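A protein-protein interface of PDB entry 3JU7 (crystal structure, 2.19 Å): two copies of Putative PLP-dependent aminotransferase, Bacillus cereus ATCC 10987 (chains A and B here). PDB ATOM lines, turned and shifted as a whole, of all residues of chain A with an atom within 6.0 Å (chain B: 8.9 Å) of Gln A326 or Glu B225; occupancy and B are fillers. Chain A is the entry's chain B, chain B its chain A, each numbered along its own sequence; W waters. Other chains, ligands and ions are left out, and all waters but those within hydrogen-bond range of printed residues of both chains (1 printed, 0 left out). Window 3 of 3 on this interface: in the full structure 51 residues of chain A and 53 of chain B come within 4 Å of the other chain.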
ATOM      1  N   THR A  87      33.017  12.366   6.659  1.00  0.00           N
ATOM      2  CA  THR A  87      33.286  13.250   5.542  1.00  0.00           C
ATOM      3  C   THR A  87      32.641  12.671   4.277  1.00  0.00           C
ATOM      4  O   THR A  87      32.061  11.604   4.314  1.00  0.00           O
ATOM      5  CB  THR A  87      34.784  13.414   5.292  1.00  0.00           C
ATOM      6  OG1 THR A  87      34.958  14.385   4.267  1.00  0.00           O
ATOM      7  CG2 THR A  87      35.428  12.065   4.882  1.00  0.00           C
ATOM      8  N   PRO A  89      32.611  10.865   0.633  1.00  0.00           N
ATOM      9  CA  PRO A  89      33.544   9.857   0.063  1.00  0.00           C
ATOM     10  C   PRO A  89      34.664  10.333  -0.846  1.00  0.00           C
ATOM     11  O   PRO A  89      35.628   9.601  -1.023  1.00  0.00           O
ATOM     12  CB  PRO A  89      32.614   8.897  -0.657  1.00  0.00           C
ATOM     13  CG  PRO A  89      31.414   8.901   0.233  1.00  0.00           C
ATOM     14  CD  PRO A  89      31.225  10.358   0.636  1.00  0.00           C
ATOM     15  N   SER A 320      25.676   9.360   6.860  1.00  0.00           N
ATOM     16  CA  SER A 320      25.228   8.107   7.439  1.00  0.00           C
ATOM     17  C   SER A 320      24.689   7.255   6.287  1.00  0.00           C
ATOM     18  O   SER A 320      23.615   7.542   5.733  1.00  0.00           O
ATOM     19  CB  SER A 320      24.164   8.353   8.533  1.00  0.00           C
ATOM     20  OG  SER A 320      23.492   7.163   8.969  1.00  0.00           O
ATOM     21  N   PRO A 321      25.434   6.204   5.910  1.00  0.00           N
ATOM     22  CA  PRO A 321      26.673   5.750   6.540  1.00  0.00           C
ATOM     23  C   PRO A 321      27.849   6.712   6.379  1.00  0.00           C
ATOM     24  O   PRO A 321      27.962   7.446   5.371  1.00  0.00           O
ATOM     25  CB  PRO A 321      26.967   4.454   5.820  1.00  0.00           C
ATOM     26  CG  PRO A 321      26.261   4.589   4.520  1.00  0.00           C
ATOM     27  CD  PRO A 321      25.055   5.387   4.750  1.00  0.00           C
ATOM     28  N   SER A 322      28.702   6.734   7.390  1.00  0.00           N
ATOM     29  CA  SER A 322      29.945   7.441   7.266  1.00  0.00           C
ATOM     30  C   SER A 322      30.863   6.577   6.426  1.00  0.00           C
ATOM     31  O   SER A 322      30.534   5.416   6.126  1.00  0.00           O
ATOM     32  CB  SER A 322      30.563   7.724   8.643  1.00  0.00           C
ATOM     33  OG  SER A 322      29.936   8.862   9.195  1.00  0.00           O
ATOM     34  N   CYS A 323      32.027   7.126   6.075  1.00  0.00           N
ATOM     35  CA  CYS A 323      32.917   6.444   5.154  1.00  0.00           C
ATOM     36  C   CYS A 323      33.296   5.054   5.632  1.00  0.00           C
ATOM     37  O   CYS A 323      33.260   4.078   4.843  1.00  0.00           O
ATOM     38  CB  CYS A 323      34.155   7.274   4.868  1.00  0.00           C
ATOM     39  SG  CYS A 323      33.830   8.762   3.839  1.00  0.00           S
ATOM     40  N   HIS A 324      33.605   4.931   6.919  1.00  0.00           N
ATOM     41  CA  HIS A 324      34.060   3.625   7.436  1.00  0.00           C
ATOM     42  C   HIS A 324      32.966   2.550   7.388  1.00  0.00           C
ATOM     43  O   HIS A 324      33.238   1.348   7.487  1.00  0.00           O
ATOM     44  CB  HIS A 324      34.679   3.767   8.842  1.00  0.00           C
ATOM     45  CG  HIS A 324      33.686   3.893   9.953  1.00  0.00           C
ATOM     46  ND1 HIS A 324      33.087   5.088  10.292  1.00  0.00           N
ATOM     47  CD2 HIS A 324      33.235   2.978  10.849  1.00  0.00           C
ATOM     48  CE1 HIS A 324      32.267   4.889  11.311  1.00  0.00           C
ATOM     49  NE2 HIS A 324      32.342   3.617  11.674  1.00  0.00           N
ATOM     50  N   GLN A 325      31.727   2.995   7.279  1.00  0.00           N
ATOM     51  CA  GLN A 325      30.589   2.117   7.234  1.00  0.00           C
ATOM     52  C   GLN A 325      30.177   1.829   5.793  1.00  0.00           C
ATOM     53  O   GLN A 325      29.223   1.077   5.553  1.00  0.00           O
ATOM     54  CB  GLN A 325      29.430   2.787   7.983  1.00  0.00           C
ATOM     55  CG  GLN A 325      29.773   3.136   9.419  1.00  0.00           C
ATOM     56  CD  GLN A 325      28.710   3.960  10.091  1.00  0.00           C
ATOM     57  OE1 GLN A 325      28.218   4.918   9.510  1.00  0.00           O
ATOM     58  NE2 GLN A 325      28.372   3.615  11.356  1.00  0.00           N
ATOM     59  N   GLN A 326      30.833   2.460   4.823  1.00  0.00           N
ATOM     60  CA  GLN A 326      30.506   2.197   3.424  1.00  0.00           C
ATOM     61  C   GLN A 326      31.318   1.038   2.871  1.00  0.00           C
ATOM     62  O   GLN A 326      32.414   0.739   3.318  1.00  0.00           O
ATOM     63  CB  GLN A 326      30.701   3.446   2.584  1.00  0.00           C
ATOM     64  CG  GLN A 326      29.729   4.517   2.988  1.00  0.00           C
ATOM     65  CD  GLN A 326      29.765   5.753   2.143  1.00  0.00           C
ATOM     66  OE1 GLN A 326      30.127   5.721   0.965  1.00  0.00           O
ATOM     67  NE2 GLN A 326      29.364   6.863   2.740  1.00  0.00           N
ATOM     68  N   VAL A 327      30.740   0.379   1.892  1.00  0.00           N
ATOM     69  CA  VAL A 327      31.328  -0.810   1.300  1.00  0.00           C
ATOM     70  C   VAL A 327      32.797  -0.644   0.985  1.00  0.00           C
ATOM     71  O   VAL A 327      33.627  -1.435   1.420  1.00  0.00           O
ATOM     72  CB  VAL A 327      30.540  -1.220   0.052  1.00  0.00           C
ATOM     73  CG1 VAL A 327      31.321  -2.177  -0.810  1.00  0.00           C
ATOM     74  CG2 VAL A 327      29.244  -1.817   0.479  1.00  0.00           C
ATOM     75  N   LEU A 328      33.138   0.396   0.247  1.00  0.00           N
ATOM     76  CA  LEU A 328      34.488   0.493  -0.228  1.00  0.00           C
ATOM     77  C   LEU A 328      35.540   0.701   0.883  1.00  0.00           C
ATOM     78  O   LEU A 328      36.677   0.227   0.753  1.00  0.00           O
ATOM     79  CB  LEU A 328      34.588   1.578  -1.306  1.00  0.00           C
ATOM     80  CG  LEU A 328      35.932   1.475  -2.020  1.00  0.00           C
ATOM     81  CD1 LEU A 328      35.944   0.260  -2.972  1.00  0.00           C
ATOM     82  CD2 LEU A 328      36.268   2.749  -2.735  1.00  0.00           C
ATOM     83  N   PHE A 329      35.183   1.392   1.960  1.00  0.00           N
ATOM     84  CA  PHE A 329      36.199   1.824   2.929  1.00  0.00           C
ATOM     85  C   PHE A 329      36.199   1.020   4.229  1.00  0.00           C
ATOM     86  O   PHE A 329      36.988   1.299   5.125  1.00  0.00           O
ATOM     87  CB  PHE A 329      36.016   3.310   3.285  1.00  0.00           C
ATOM     88  CG  PHE A 329      35.769   4.190   2.104  1.00  0.00           C
ATOM     89  CD1 PHE A 329      36.817   4.551   1.268  1.00  0.00           C
ATOM     90  CD2 PHE A 329      34.472   4.663   1.815  1.00  0.00           C
ATOM     91  CE1 PHE A 329      36.581   5.373   0.161  1.00  0.00           C
ATOM     92  CE2 PHE A 329      34.231   5.489   0.710  1.00  0.00           C
ATOM     93  CZ  PHE A 329      35.285   5.847  -0.115  1.00  0.00           C
ATOM     94  N   ARG A 330      35.301   0.048   4.315  1.00  0.00           N
ATOM     95  CA  ARG A 330      35.006  -0.647   5.567  1.00  0.00           C
ATOM     96  C   ARG A 330      36.182  -1.361   6.169  1.00  0.00           C
ATOM     97  O   ARG A 330      36.128  -1.695   7.310  1.00  0.00           O
ATOM     98  CB  ARG A 330      33.940  -1.699   5.341  1.00  0.00           C
ATOM     99  CG  ARG A 330      34.466  -2.948   4.697  1.00  0.00           C
ATOM    100  CD  ARG A 330      33.346  -3.790   4.172  1.00  0.00           C
ATOM    101  NE  ARG A 330      33.881  -5.024   3.622  1.00  0.00           N
ATOM    102  CZ  ARG A 330      34.246  -5.207   2.351  1.00  0.00           C
ATOM    103  NH1 ARG A 330      34.116  -4.260   1.439  1.00  0.00           N
ATOM    104  NH2 ARG A 330      34.732  -6.370   1.987  1.00  0.00           N
ATOM    105  N   ASN A 331      37.237  -1.637   5.406  1.00  0.00           N
ATOM    106  CA  ASN A 331      38.366  -2.397   5.980  1.00  0.00           C
ATOM    107  C   ASN A 331      39.619  -1.602   6.249  1.00  0.00           C
ATOM    108  O   ASN A 331      40.646  -2.189   6.654  1.00  0.00           O
ATOM    109  CB  ASN A 331      38.682  -3.611   5.126  1.00  0.00           C
ATOM    110  CG  ASN A 331      37.669  -4.698   5.323  1.00  0.00           C
ATOM    111  OD1 ASN A 331      37.151  -4.845   6.408  1.00  0.00           O
ATOM    112  ND2 ASN A 331      37.384  -5.465   4.286  1.00  0.00           N
ATOM    113  N   ARG B 214      29.086   5.283 -12.788  1.00  0.00           N
ATOM    114  CA  ARG B 214      29.092   5.315 -11.351  1.00  0.00           C
ATOM    115  C   ARG B 214      30.468   5.708 -10.838  1.00  0.00           C
ATOM    116  O   ARG B 214      30.544   6.493  -9.903  1.00  0.00           O
ATOM    117  CB  ARG B 214      28.731   3.960 -10.783  1.00  0.00           C
ATOM    118  CG  ARG B 214      27.255   3.557 -10.959  1.00  0.00           C
ATOM    119  CD  ARG B 214      27.051   2.276 -10.142  1.00  0.00           C
ATOM    120  NE  ARG B 214      25.748   1.694 -10.371  1.00  0.00           N
ATOM    121  CZ  ARG B 214      25.176   0.782  -9.599  1.00  0.00           C
ATOM    122  NH1 ARG B 214      25.780   0.325  -8.517  1.00  0.00           N
ATOM    123  NH2 ARG B 214      23.960   0.358  -9.899  1.00  0.00           N
ATOM    124  N   ASN B 217      31.130   9.271 -10.554  1.00  0.00           N
ATOM    125  CA  ASN B 217      30.295   9.882  -9.525  1.00  0.00           C
ATOM    126  C   ASN B 217      30.565   9.133  -8.221  1.00  0.00           C
ATOM    127  O   ASN B 217      29.650   8.606  -7.572  1.00  0.00           O
ATOM    128  CB  ASN B 217      28.794   9.803  -9.929  1.00  0.00           C
ATOM    129  CG  ASN B 217      27.863  10.528  -8.939  1.00  0.00           C
ATOM    130  OD1 ASN B 217      28.190  11.598  -8.393  1.00  0.00           O
ATOM    131  ND2 ASN B 217      26.700   9.952  -8.723  1.00  0.00           N
ATOM    132  N   PHE B 218      31.854   9.051  -7.864  1.00  0.00           N
ATOM    133  CA  PHE B 218      32.286   8.561  -6.563  1.00  0.00           C
ATOM    134  C   PHE B 218      31.972   7.089  -6.267  1.00  0.00           C
ATOM    135  O   PHE B 218      31.882   6.689  -5.094  1.00  0.00           O
ATOM    136  CB  PHE B 218      31.694   9.461  -5.452  1.00  0.00           C
ATOM    137  CG  PHE B 218      31.818  10.934  -5.742  1.00  0.00           C
ATOM    138  CD1 PHE B 218      33.032  11.581  -5.572  1.00  0.00           C
ATOM    139  CD2 PHE B 218      30.746  11.657  -6.204  1.00  0.00           C
ATOM    140  CE1 PHE B 218      33.171  12.912  -5.842  1.00  0.00           C
ATOM    141  CE2 PHE B 218      30.891  13.010  -6.484  1.00  0.00           C
ATOM    142  CZ  PHE B 218      32.121  13.629  -6.295  1.00  0.00           C
ATOM    143  N   GLY B 219      31.823   6.267  -7.300  1.00  0.00           N
ATOM    144  CA  GLY B 219      31.453   4.861  -7.077  1.00  0.00           C
ATOM    145  C   GLY B 219      30.062   4.640  -6.480  1.00  0.00           C
ATOM    146  O   GLY B 219      29.786   3.587  -5.900  1.00  0.00           O
ATOM    147  N   PHE B 220      29.197   5.642  -6.601  1.00  0.00           N
ATOM    148  CA  PHE B 220      27.894   5.625  -5.954  1.00  0.00           C
ATOM    149  C   PHE B 220      26.922   4.731  -6.628  1.00  0.00           C
ATOM    150  O   PHE B 220      26.840   4.742  -7.833  1.00  0.00           O
ATOM    151  CB  PHE B 220      27.254   7.021  -5.939  1.00  0.00           C
ATOM    152  CG  PHE B 220      27.800   7.938  -4.902  1.00  0.00           C
ATOM    153  CD1 PHE B 220      28.616   7.472  -3.867  1.00  0.00           C
ATOM    154  CD2 PHE B 220      27.436   9.289  -4.915  1.00  0.00           C
ATOM    155  CE1 PHE B 220      29.106   8.371  -2.866  1.00  0.00           C
ATOM    156  CE2 PHE B 220      27.922  10.179  -3.943  1.00  0.00           C
ATOM    157  CZ  PHE B 220      28.745   9.716  -2.921  1.00  0.00           C
ATOM    158  N   ASP B 221      26.209   3.969  -5.815  1.00  0.00           N
ATOM    159  CA  ASP B 221      25.050   3.159  -6.207  1.00  0.00           C
ATOM    160  C   ASP B 221      23.843   4.039  -6.026  1.00  0.00           C
ATOM    161  O   ASP B 221      23.989   5.237  -5.812  1.00  0.00           O
ATOM    162  CB  ASP B 221      24.935   1.859  -5.363  1.00  0.00           C
ATOM    163  CG  ASP B 221      24.649   2.101  -3.862  1.00  0.00           C
ATOM    164  OD1 ASP B 221      24.394   3.249  -3.449  1.00  0.00           O
ATOM    165  OD2 ASP B 221      24.691   1.114  -3.082  1.00  0.00           O
ATOM    166  N   THR B 222      22.648   3.469  -6.104  1.00  0.00           N
ATOM    167  CA  THR B 222      21.458   4.285  -6.110  1.00  0.00           C
ATOM    168  C   THR B 222      21.146   4.855  -4.723  1.00  0.00           C
ATOM    169  O   THR B 222      20.283   5.704  -4.601  1.00  0.00           O
ATOM    170  CB  THR B 222      20.245   3.503  -6.627  1.00  0.00           C
ATOM    171  OG1 THR B 222      20.008   2.400  -5.748  1.00  0.00           O
ATOM    172  CG2 THR B 222      20.540   2.990  -8.048  1.00  0.00           C
ATOM    173  N   ASN B 223      21.828   4.388  -3.684  1.00  0.00           N
ATOM    174  CA  ASN B 223      21.732   5.038  -2.379  1.00  0.00           C
ATOM    175  C   ASN B 223      22.783   6.129  -2.145  1.00  0.00           C
ATOM    176  O   ASN B 223      22.891   6.656  -1.035  1.00  0.00           O
ATOM    177  CB  ASN B 223      21.838   4.002  -1.277  1.00  0.00           C
ATOM    178  CG  ASN B 223      20.698   3.037  -1.286  1.00  0.00           C
ATOM    179  OD1 ASN B 223      19.522   3.414  -1.400  1.00  0.00           O
ATOM    180  ND2 ASN B 223      21.028   1.782  -1.180  1.00  0.00           N
ATOM    181  N   ARG B 224      23.537   6.464  -3.190  1.00  0.00           N
ATOM    182  CA  ARG B 224      24.630   7.417  -3.085  1.00  0.00           C
ATOM    183  C   ARG B 224      25.587   6.941  -2.010  1.00  0.00           C
ATOM    184  O   ARG B 224      26.045   7.712  -1.194  1.00  0.00           O
ATOM    185  CB  ARG B 224      24.133   8.847  -2.820  1.00  0.00           C
ATOM    186  CG  ARG B 224      23.136   9.315  -3.915  1.00  0.00           C
ATOM    187  CD  ARG B 224      22.664  10.739  -3.686  1.00  0.00           C
ATOM    188  NE  ARG B 224      21.856  10.799  -2.477  1.00  0.00           N
ATOM    189  CZ  ARG B 224      20.532  10.673  -2.434  1.00  0.00           C
ATOM    190  NH1 ARG B 224      19.816  10.532  -3.544  1.00  0.00           N
ATOM    191  NH2 ARG B 224      19.915  10.729  -1.264  1.00  0.00           N
ATOM    192  N   GLU B 225      25.835   5.639  -2.020  1.00  0.00           N
ATOM    193  CA  GLU B 225      26.851   5.009  -1.203  1.00  0.00           C
ATOM    194  C   GLU B 225      27.991   4.531  -2.108  1.00  0.00           C
ATOM    195  O   GLU B 225      27.748   4.022  -3.207  1.00  0.00           O
ATOM    196  CB  GLU B 225      26.264   3.813  -0.467  1.00  0.00           C
ATOM    197  CG  GLU B 225      27.370   2.915   0.162  1.00  0.00           C
ATOM    198  CD  GLU B 225      26.856   1.912   1.182  1.00  0.00           C
ATOM    199  OE1 GLU B 225      25.611   1.901   1.426  1.00  0.00           O
ATOM    200  OE2 GLU B 225      27.716   1.165   1.735  1.00  0.00           O
ATOM    201  N   CYS B 226      29.213   4.627  -1.617  1.00  0.00           N
ATOM    202  CA  CYS B 226      30.380   4.242  -2.391  1.00  0.00           C
ATOM    203  C   CYS B 226      30.677   2.745  -2.299  1.00  0.00           C
ATOM    204  O   CYS B 226      31.119   2.229  -1.258  1.00  0.00           O
ATOM    205  CB  CYS B 226      31.618   4.981  -1.895  1.00  0.00           C
ATOM    206  SG  CYS B 226      33.097   4.521  -2.844  1.00  0.00           S
ATOM    207  N   THR B 227      30.495   2.053  -3.412  1.00  0.00           N
ATOM    208  CA  THR B 227      30.692   0.593  -3.444  1.00  0.00           C
ATOM    209  C   THR B 227      31.814   0.115  -4.352  1.00  0.00           C
ATOM    210  O   THR B 227      32.032  -1.086  -4.440  1.00  0.00           O
ATOM    211  CB  THR B 227      29.437  -0.103  -3.916  1.00  0.00           C
ATOM    212  OG1 THR B 227      29.265   0.179  -5.301  1.00  0.00           O
ATOM    213  CG2 THR B 227      28.239   0.372  -3.114  1.00  0.00           C
ATOM    214  N   MET B 228      32.494   1.050  -5.015  1.00  0.00           N
ATOM    215  CA  MET B 228      33.624   0.749  -5.877  1.00  0.00           C
ATOM    216  C   MET B 228      34.560   1.969  -6.013  1.00  0.00           C
ATOM    217  O   MET B 228      34.185   3.105  -5.725  1.00  0.00           O
ATOM    218  CB  MET B 228      33.124   0.377  -7.277  1.00  0.00           C
ATOM    219  CG  MET B 228      32.290   1.478  -7.953  1.00  0.00           C
ATOM    220  SD  MET B 228      31.568   0.944  -9.709  1.00  0.00           S
ATOM    221  CE  MET B 228      33.027  -0.047 -10.360  1.00  0.00           C
HETATM  222  O   HOH W   1      27.357   0.360   4.220  1.00  0.00           O
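The side-chain carboxylate (OE2) of Glu B225 lies within hydrogen-bond range of the backbone NH (N) of Val A327 (3.1 Å).
OE1 of Gln A326 is in hydrogen-bond range of N of Cys B226 (2.9 Å).
The backbone carbonyl oxygen of Cys B226 sits at hydrogen-bond distance from the backbone NH of Leu A328 (3.1 Å).
The backbone carbonyl oxygen (O) of Phe B218 lies within hydrogen-bond range of the side-chain sulfur (SG) of Cys B226.
O of Gly B219 is in hydrogen-bond range of N of Thr B227 (3.0 Å).
N of Glu B225 lies within hydrogen-bond range of OD1 of Asp B221 (3.1 Å).
The side-chain sulfur (SG) of Cys B226 is in hydrogen-bond range of the backbone carbonyl oxygen (O) of Met B228 (3.4 Å).
NE2 of Gln A326 sits at hydrogen-bond distance from O of Pro A321, at 3.0 Å.
O of Val A327 sits at hydrogen-bond distance from NH1 of Arg A330.
CG of Pro A89 touches CE1 of Phe B220, at 3.9 Å.
CA of Gln A326 touches OE2 of Glu B225 (3.4 Å).
Cys B226 touches Val A327 (O to N, 3.7 Å).
Thr B227 touches Val A327 (O to CG1, 3.9 Å).
CD2 of Leu A328 touches O of Met B228, 3.7 Å away.
Phe A329 touches Cys B226 (CE2 to CB, 3.7 Å).
Of chain A, only Gln A326 (3.4 Å) and Val A327 (3.1 Å) come within 4 Å of Glu B225.
Of the printed residues of chain A, Met B228 touches Leu A328 (3.7 Å).
Printed residues of chain A within 4 Å of Phe B220: Pro A89 (3.9 Å).
Of the printed residues of chain A, Thr B227 touches Val A327.
Of the printed residues of chain B, Val A327 touches Glu B225, Cys B226 and Thr B227.
Gly B219 touches none of the printed residues of chain A.
Ser A322 touches none of the printed residues of chain B.
The nearest residue of chain B that does not touch Gln A326 is Phe B220 (4.8 Å).
Of the 13 printed residues of chain B, 5 touch a printed residue of chain A.
Printed residues of chain B that touch a printed residue of chain A: Phe B220, Glu B225, Cys B226, Thr B227 and Met B228.
Hydrophobic or aromatic side chains of chain B that line the printed part of chain A: Phe B220.
Of the 14 printed residues of chain A, 5 touch a printed residue of chain B.
Hydrophobic or aromatic side chains of chain A within 4 Å of the printed part of chain B: Pro A89, Val A327, Leu A328 and Phe A329.
Among the printed residues, no Asp or Glu carboxylate lies within 4 Å of a Lys or Arg side-chain nitrogen of the other chain.
No position is printed for both chains.
Water W1 lies within hydrogen-bond range of O of Gln A325 (2.4 Å) and OE2 of Glu B225 (2.6 Å).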
